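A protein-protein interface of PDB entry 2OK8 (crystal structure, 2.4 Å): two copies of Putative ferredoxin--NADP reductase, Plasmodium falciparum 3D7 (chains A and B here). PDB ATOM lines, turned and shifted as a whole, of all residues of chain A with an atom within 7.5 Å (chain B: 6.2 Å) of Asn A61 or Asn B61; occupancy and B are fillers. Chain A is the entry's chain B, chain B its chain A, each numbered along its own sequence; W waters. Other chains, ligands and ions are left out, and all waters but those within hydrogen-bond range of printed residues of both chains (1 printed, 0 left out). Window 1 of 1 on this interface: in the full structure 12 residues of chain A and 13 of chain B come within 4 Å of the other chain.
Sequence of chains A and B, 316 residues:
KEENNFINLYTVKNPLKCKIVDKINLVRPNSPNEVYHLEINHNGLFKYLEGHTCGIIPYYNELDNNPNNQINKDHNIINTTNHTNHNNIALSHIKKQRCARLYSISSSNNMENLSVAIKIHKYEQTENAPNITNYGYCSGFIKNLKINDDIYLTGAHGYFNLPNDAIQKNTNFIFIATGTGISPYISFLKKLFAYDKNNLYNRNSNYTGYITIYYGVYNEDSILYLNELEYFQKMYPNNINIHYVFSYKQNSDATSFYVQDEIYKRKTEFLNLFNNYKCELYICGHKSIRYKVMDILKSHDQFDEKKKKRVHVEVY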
ATOM      1  N   LYS A  17     -18.603   1.726  11.494  1.00  0.00           N
ATOM      2  CA  LYS A  17     -18.637   2.128  10.100  1.00  0.00           C
ATOM      3  C   LYS A  17     -18.571   3.658  10.058  1.00  0.00           C
ATOM      4  O   LYS A  17     -19.306   4.345  10.787  1.00  0.00           O
ATOM      5  CB  LYS A  17     -19.907   1.596   9.442  1.00  0.00           C
ATOM      6  CG  LYS A  17     -19.942   1.626   7.913  1.00  0.00           C
ATOM      7  CD  LYS A  17     -21.393   1.757   7.476  1.00  0.00           C
ATOM      8  CE  LYS A  17     -21.609   1.464   6.005  1.00  0.00           C
ATOM      9  NZ  LYS A  17     -22.960   1.945   5.587  1.00  0.00           N
ATOM     10  N   ILE A  57      -9.548  -1.547   9.677  1.00  0.00           N
ATOM     11  CA  ILE A  57      -9.650  -2.905   9.143  1.00  0.00           C
ATOM     12  C   ILE A  57      -9.669  -2.866   7.623  1.00  0.00           C
ATOM     13  O   ILE A  57     -10.710  -2.612   7.021  1.00  0.00           O
ATOM     14  CB  ILE A  57     -10.895  -3.681   9.653  1.00  0.00           C
ATOM     15  CG1 ILE A  57     -11.062  -3.539  11.172  1.00  0.00           C
ATOM     16  CG2 ILE A  57     -10.768  -5.160   9.271  1.00  0.00           C
ATOM     17  CD1 ILE A  57     -12.308  -4.242  11.727  1.00  0.00           C
ATOM     18  N   PRO A  58      -8.519  -3.108   6.989  1.00  0.00           N
ATOM     19  CA  PRO A  58      -8.544  -3.025   5.542  1.00  0.00           C
ATOM     20  C   PRO A  58      -9.561  -3.955   4.864  1.00  0.00           C
ATOM     21  O   PRO A  58      -9.680  -5.127   5.220  1.00  0.00           O
ATOM     22  CB  PRO A  58      -7.112  -3.382   5.114  1.00  0.00           C
ATOM     23  CG  PRO A  58      -6.338  -3.650   6.345  1.00  0.00           C
ATOM     24  CD  PRO A  58      -7.194  -3.428   7.537  1.00  0.00           C
ATOM     25  N   TYR A  59     -10.280  -3.395   3.893  1.00  0.00           N
ATOM     26  CA  TYR A  59     -11.100  -4.134   2.928  1.00  0.00           C
ATOM     27  C   TYR A  59     -12.367  -4.734   3.527  1.00  0.00           C
ATOM     28  O   TYR A  59     -13.082  -5.487   2.857  1.00  0.00           O
ATOM     29  CB  TYR A  59     -10.287  -5.222   2.238  1.00  0.00           C
ATOM     30  CG  TYR A  59      -9.162  -4.738   1.360  1.00  0.00           C
ATOM     31  CD1 TYR A  59      -7.838  -4.802   1.791  1.00  0.00           C
ATOM     32  CD2 TYR A  59      -9.416  -4.236   0.086  1.00  0.00           C
ATOM     33  CE1 TYR A  59      -6.795  -4.381   0.971  1.00  0.00           C
ATOM     34  CE2 TYR A  59      -8.382  -3.805  -0.740  1.00  0.00           C
ATOM     35  CZ  TYR A  59      -7.075  -3.888  -0.294  1.00  0.00           C
ATOM     36  OH  TYR A  59      -6.046  -3.459  -1.114  1.00  0.00           O
ATOM     37  N   TYR A  60     -12.633  -4.387   4.781  1.00  0.00           N
ATOM     38  CA  TYR A  60     -13.818  -4.828   5.494  1.00  0.00           C
ATOM     39  C   TYR A  60     -15.083  -4.361   4.787  1.00  0.00           C
ATOM     40  O   TYR A  60     -15.108  -3.302   4.159  1.00  0.00           O
ATOM     41  CB  TYR A  60     -13.796  -4.270   6.915  1.00  0.00           C
ATOM     42  CG  TYR A  60     -14.789  -4.904   7.858  1.00  0.00           C
ATOM     43  CD1 TYR A  60     -14.394  -5.902   8.741  1.00  0.00           C
ATOM     44  CD2 TYR A  60     -16.123  -4.503   7.876  1.00  0.00           C
ATOM     45  CE1 TYR A  60     -15.296  -6.479   9.613  1.00  0.00           C
ATOM     46  CE2 TYR A  60     -17.030  -5.072   8.745  1.00  0.00           C
ATOM     47  CZ  TYR A  60     -16.613  -6.063   9.604  1.00  0.00           C
ATOM     48  OH  TYR A  60     -17.516  -6.633  10.470  1.00  0.00           O
ATOM     49  N   ASN A  61     -16.123  -5.178   4.903  1.00  0.00           N
ATOM     50  CA  ASN A  61     -17.460  -4.894   4.415  1.00  0.00           C
ATOM     51  C   ASN A  61     -18.448  -5.625   5.329  1.00  0.00           C
ATOM     52  O   ASN A  61     -18.300  -6.821   5.567  1.00  0.00           O
ATOM     53  CB  ASN A  61     -17.589  -5.380   2.975  1.00  0.00           C
ATOM     54  CG  ASN A  61     -18.806  -4.794   2.242  1.00  0.00           C
ATOM     55  OD1 ASN A  61     -19.260  -3.674   2.510  1.00  0.00           O
ATOM     56  ND2 ASN A  61     -19.328  -5.564   1.293  1.00  0.00           N
ATOM     57  N   GLU A  62     -19.427  -4.893   5.857  1.00  0.00           N
ATOM     58  CA  GLU A  62     -20.491  -5.439   6.709  1.00  0.00           C
ATOM     59  C   GLU A  62     -21.128  -6.710   6.171  1.00  0.00           C
ATOM     60  O   GLU A  62     -21.444  -6.796   4.977  1.00  0.00           O
ATOM     61  CB  GLU A  62     -21.600  -4.406   6.895  1.00  0.00           C
ATOM     62  CG  GLU A  62     -21.385  -3.477   8.057  1.00  0.00           C
ATOM     63  CD  GLU A  62     -22.457  -2.415   8.155  1.00  0.00           C
ATOM     64  OE1 GLU A  62     -22.954  -1.960   7.102  1.00  0.00           O
ATOM     65  OE2 GLU A  62     -22.798  -2.027   9.292  1.00  0.00           O
ATOM     66  N   LEU A  63     -21.315  -7.683   7.064  1.00  0.00           N
ATOM     67  CA  LEU A  63     -22.056  -8.906   6.758  1.00  0.00           C
ATOM     68  C   LEU A  63     -23.326  -8.890   7.593  1.00  0.00           C
ATOM     69  O   LEU A  63     -24.043  -7.890   7.600  1.00  0.00           O
ATOM     70  CB  LEU A  63     -21.231 -10.168   7.059  1.00  0.00           C
ATOM     71  CG  LEU A  63     -21.384 -11.458   6.230  1.00  0.00           C
ATOM     72  CD1 LEU A  63     -22.846 -11.830   5.970  1.00  0.00           C
ATOM     73  CD2 LEU A  63     -20.619 -11.377   4.912  1.00  0.00           C
ATOM     74  N   TYR A 137      -0.377  -4.392   3.099  1.00  0.00           N
ATOM     75  CA  TYR A 137      -1.783  -4.746   3.124  1.00  0.00           C
ATOM     76  C   TYR A 137      -2.705  -3.521   3.302  1.00  0.00           C
ATOM     77  O   TYR A 137      -3.491  -3.214   2.415  1.00  0.00           O
ATOM     78  CB  TYR A 137      -2.039  -5.812   4.199  1.00  0.00           C
ATOM     79  CG  TYR A 137      -3.439  -6.341   4.241  1.00  0.00           C
ATOM     80  CD1 TYR A 137      -4.062  -6.798   3.088  1.00  0.00           C
ATOM     81  CD2 TYR A 137      -4.139  -6.420   5.440  1.00  0.00           C
ATOM     82  CE1 TYR A 137      -5.358  -7.296   3.120  1.00  0.00           C
ATOM     83  CE2 TYR A 137      -5.436  -6.920   5.479  1.00  0.00           C
ATOM     84  CZ  TYR A 137      -6.032  -7.362   4.315  1.00  0.00           C
ATOM     85  OH  TYR A 137      -7.310  -7.868   4.333  1.00  0.00           O
ATOM     86  N   PHE A 141      -4.782  -0.701   0.524  1.00  0.00           N
ATOM     87  CA  PHE A 141      -6.167  -0.303   0.796  1.00  0.00           C
ATOM     88  C   PHE A 141      -6.329   1.229   0.876  1.00  0.00           C
ATOM     89  O   PHE A 141      -7.215   1.790   0.259  1.00  0.00           O
ATOM     90  CB  PHE A 141      -6.654  -0.976   2.085  1.00  0.00           C
ATOM     91  CG  PHE A 141      -8.014  -0.498   2.565  1.00  0.00           C
ATOM     92  CD1 PHE A 141      -9.154  -0.716   1.801  1.00  0.00           C
ATOM     93  CD2 PHE A 141      -8.143   0.146   3.799  1.00  0.00           C
ATOM     94  CE1 PHE A 141     -10.397  -0.281   2.235  1.00  0.00           C
ATOM     95  CE2 PHE A 141      -9.368   0.605   4.234  1.00  0.00           C
ATOM     96  CZ  PHE A 141     -10.507   0.388   3.455  1.00  0.00           C
ATOM     97  N   ASP A 150     -16.493   4.002   2.611  1.00  0.00           N
ATOM     98  CA  ASP A 150     -16.622   3.555   3.987  1.00  0.00           C
ATOM     99  C   ASP A 150     -15.295   3.043   4.498  1.00  0.00           C
ATOM    100  O   ASP A 150     -14.461   2.520   3.749  1.00  0.00           O
ATOM    101  CB  ASP A 150     -17.663   2.433   4.118  1.00  0.00           C
ATOM    102  CG  ASP A 150     -19.089   2.928   3.929  1.00  0.00           C
ATOM    103  OD1 ASP A 150     -19.441   4.024   4.444  1.00  0.00           O
ATOM    104  OD2 ASP A 150     -19.862   2.201   3.270  1.00  0.00           O
ATOM    105  N   TYR A 152     -13.876   1.160   8.312  1.00  0.00           N
ATOM    106  CA  TYR A 152     -14.321   0.586   9.565  1.00  0.00           C
ATOM    107  C   TYR A 152     -13.240   0.725  10.621  1.00  0.00           C
ATOM    108  O   TYR A 152     -12.124   0.257  10.434  1.00  0.00           O
ATOM    109  CB  TYR A 152     -14.669  -0.895   9.359  1.00  0.00           C
ATOM    110  CG  TYR A 152     -15.906  -1.108   8.514  1.00  0.00           C
ATOM    111  CD1 TYR A 152     -15.825  -1.086   7.119  1.00  0.00           C
ATOM    112  CD2 TYR A 152     -17.159  -1.311   9.109  1.00  0.00           C
ATOM    113  CE1 TYR A 152     -16.942  -1.265   6.334  1.00  0.00           C
ATOM    114  CE2 TYR A 152     -18.297  -1.506   8.322  1.00  0.00           C
ATOM    115  CZ  TYR A 152     -18.175  -1.479   6.937  1.00  0.00           C
ATOM    116  OH  TYR A 152     -19.270  -1.651   6.130  1.00  0.00           O
ATOM    117  N   TYR B  59     -14.564 -11.049   6.000  1.00  0.00           N
ATOM    118  CA  TYR B  59     -15.252  -9.794   5.647  1.00  0.00           C
ATOM    119  C   TYR B  59     -14.633  -9.051   4.497  1.00  0.00           C
ATOM    120  O   TYR B  59     -15.074  -7.962   4.154  1.00  0.00           O
ATOM    121  CB  TYR B  59     -15.381  -8.859   6.845  1.00  0.00           C
ATOM    122  CG  TYR B  59     -16.169  -9.439   7.990  1.00  0.00           C
ATOM    123  CD1 TYR B  59     -15.520 -10.026   9.063  1.00  0.00           C
ATOM    124  CD2 TYR B  59     -17.569  -9.399   8.001  1.00  0.00           C
ATOM    125  CE1 TYR B  59     -16.225 -10.559  10.124  1.00  0.00           C
ATOM    126  CE2 TYR B  59     -18.291  -9.938   9.067  1.00  0.00           C
ATOM    127  CZ  TYR B  59     -17.609 -10.515  10.126  1.00  0.00           C
ATOM    128  OH  TYR B  59     -18.290 -11.048  11.213  1.00  0.00           O
ATOM    129  N   TYR B  60     -13.628  -9.649   3.882  1.00  0.00           N
ATOM    130  CA  TYR B  60     -12.967  -9.026   2.762  1.00  0.00           C
ATOM    131  C   TYR B  60     -13.933  -8.696   1.631  1.00  0.00           C
ATOM    132  O   TYR B  60     -14.837  -9.467   1.301  1.00  0.00           O
ATOM    133  CB  TYR B  60     -11.887  -9.944   2.236  1.00  0.00           C
ATOM    134  CG  TYR B  60     -10.890  -9.283   1.309  1.00  0.00           C
ATOM    135  CD1 TYR B  60      -9.683  -8.785   1.808  1.00  0.00           C
ATOM    136  CD2 TYR B  60     -11.124  -9.189  -0.066  1.00  0.00           C
ATOM    137  CE1 TYR B  60      -8.739  -8.200   0.972  1.00  0.00           C
ATOM    138  CE2 TYR B  60     -10.168  -8.612  -0.923  1.00  0.00           C
ATOM    139  CZ  TYR B  60      -8.983  -8.108  -0.383  1.00  0.00           C
ATOM    140  OH  TYR B  60      -8.019  -7.528  -1.181  1.00  0.00           O
ATOM    141  N   ASN B  61     -13.702  -7.539   1.030  1.00  0.00           N
ATOM    142  CA  ASN B  61     -14.356  -7.144  -0.188  1.00  0.00           C
ATOM    143  C   ASN B  61     -13.337  -6.394  -1.026  1.00  0.00           C
ATOM    144  O   ASN B  61     -12.642  -5.528  -0.514  1.00  0.00           O
ATOM    145  CB  ASN B  61     -15.556  -6.263   0.153  1.00  0.00           C
ATOM    146  CG  ASN B  61     -16.473  -6.060  -1.016  1.00  0.00           C
ATOM    147  OD1 ASN B  61     -16.748  -6.992  -1.773  1.00  0.00           O
ATOM    148  ND2 ASN B  61     -16.954  -4.834  -1.181  1.00  0.00           N
ATOM    149  N   GLU B  62     -13.223  -6.752  -2.300  1.00  0.00           N
ATOM    150  CA  GLU B  62     -12.336  -6.058  -3.244  1.00  0.00           C
ATOM    151  C   GLU B  62     -12.593  -4.556  -3.268  1.00  0.00           C
ATOM    152  O   GLU B  62     -13.733  -4.122  -3.455  1.00  0.00           O
ATOM    153  CB  GLU B  62     -12.539  -6.594  -4.659  1.00  0.00           C
ATOM    154  CG  GLU B  62     -11.924  -7.942  -4.942  1.00  0.00           C
ATOM    155  CD  GLU B  62     -12.584  -8.622  -6.131  1.00  0.00           C
ATOM    156  OE1 GLU B  62     -13.718  -8.217  -6.482  1.00  0.00           O
ATOM    157  OE2 GLU B  62     -11.974  -9.558  -6.707  1.00  0.00           O
ATOM    158  N   ASP B 150     -19.415 -14.668  -1.588  1.00  0.00           N
ATOM    159  CA  ASP B 150     -18.004 -14.567  -1.908  1.00  0.00           C
ATOM    160  C   ASP B 150     -17.191 -14.877  -0.670  1.00  0.00           C
ATOM    161  O   ASP B 150     -17.602 -14.549   0.446  1.00  0.00           O
ATOM    162  CB  ASP B 150     -17.662 -13.157  -2.382  1.00  0.00           C
ATOM    163  CG  ASP B 150     -18.103 -12.896  -3.806  1.00  0.00           C
ATOM    164  OD1 ASP B 150     -18.060 -13.838  -4.638  1.00  0.00           O
ATOM    165  OD2 ASP B 150     -18.477 -11.736  -4.092  1.00  0.00           O
ATOM    166  N   TYR B 152     -12.774 -15.012   0.337  1.00  0.00           N
ATOM    167  CA  TYR B 152     -11.446 -14.720  -0.203  1.00  0.00           C
ATOM    168  C   TYR B 152     -10.363 -15.567   0.437  1.00  0.00           C
ATOM    169  O   TYR B 152     -10.264 -15.645   1.662  1.00  0.00           O
ATOM    170  CB  TYR B 152     -11.133 -13.233  -0.059  1.00  0.00           C
ATOM    171  CG  TYR B 152     -11.944 -12.372  -0.993  1.00  0.00           C
ATOM    172  CD1 TYR B 152     -13.277 -12.081  -0.713  1.00  0.00           C
ATOM    173  CD2 TYR B 152     -11.385 -11.851  -2.165  1.00  0.00           C
ATOM    174  CE1 TYR B 152     -14.038 -11.288  -1.557  1.00  0.00           C
ATOM    175  CE2 TYR B 152     -12.141 -11.046  -3.021  1.00  0.00           C
ATOM    176  CZ  TYR B 152     -13.468 -10.773  -2.705  1.00  0.00           C
ATOM    177  OH  TYR B 152     -14.251  -9.988  -3.525  1.00  0.00           O
HETATM  178  O   HOH W   1     -18.125  -8.970   3.936  1.00  0.00           O
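Ile A57 touches none of the printed residues of chain B. Printed residues of chain B within 4 Å of Tyr A59: Tyr B59 (3.4 Å), Tyr B60 (3.5 Å) and Asn B61 (2.8 Å). Of the printed residues of chain B, Tyr A60 touches Tyr B59 (3.5 Å). Printed residues of chain B within 4 Å of Leu A63: Tyr B59. Tyr A152 touches none of the printed residues of chain B. Printed residues of chain A within 4 Å of Tyr B59: Tyr A59 (3.4 Å), Tyr A60 (3.5 Å), Asn A61 (3.1 Å) and Leu A63 (3.6 Å). Printed residues of chain A within 4 Å of Tyr B60: Tyr A59 (3.5 Å) and Tyr A137 (3.6 Å). Asn B61 touches two residues of chain A. The nearest residue of chain A that does not touch Asn B61 is Tyr A60 (5.0 Å). The nearest printed residue of chain B that does not touch Tyr A59 is Glu B62 (4.6 Å).
The backbone carbonyl oxygen (O) of Tyr B59 is in hydrogen-bond range of the backbone NH (N) of Asn A61, 3.1 Å away. N of Asn B61 lies within hydrogen-bond range of O of Tyr A59. The backbone carbonyl oxygen of Tyr B59 lies close to the backbone carbonyl oxygen of Tyr A59.
N of Phe A141 is in hydrogen-bond range of OH of Tyr A59 (3.4 Å).
Water W1 lies within hydrogen-bond range of the backbone carbonyl oxygen (O) of Asn A61 (2.7 Å) and the backbone carbonyl oxygen (O) of Tyr B59 (3.2 Å).
Tyr B59 touches its own counterpart, Tyr A59. Tyr A59 touches Tyr B60, and with the chains exchanged Tyr A60 touches Tyr B59. Tyr A59 touches Asn B61, and with the chains exchanged Asn A61 touches Tyr B59. Asn B61 touches its own counterpart, Asn A61. Of the 8 pairs that touch across the chains among the printed residues, 6 have their exchanged pair printed and touching as well.
Hydrophobic or aromatic side chains of chain B that line the printed part of chain A: Tyr B59 and Tyr B60. Of the 12 printed residues of chain A, 5 touch a printed residue of chain B. Hydrophobic or aromatic side chains of chain A within 4 Å of the printed part of chain B: Tyr A59, Tyr A60, Leu A63 and Tyr A137. Along chain A the printed residues that touch a printed residue of chain B span positions 59 to 137.
Among the printed residues, pairs that only touch across the chains: Tyr A59 with Tyr B60 (3.5 Å), Tyr A60 with Tyr B59 (3.5 Å), Asn A61 with Asn B61 (3.5 Å), Leu A63 with Tyr B59 (3.6 Å) and Tyr A137 with Tyr B60 (3.6 Å).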
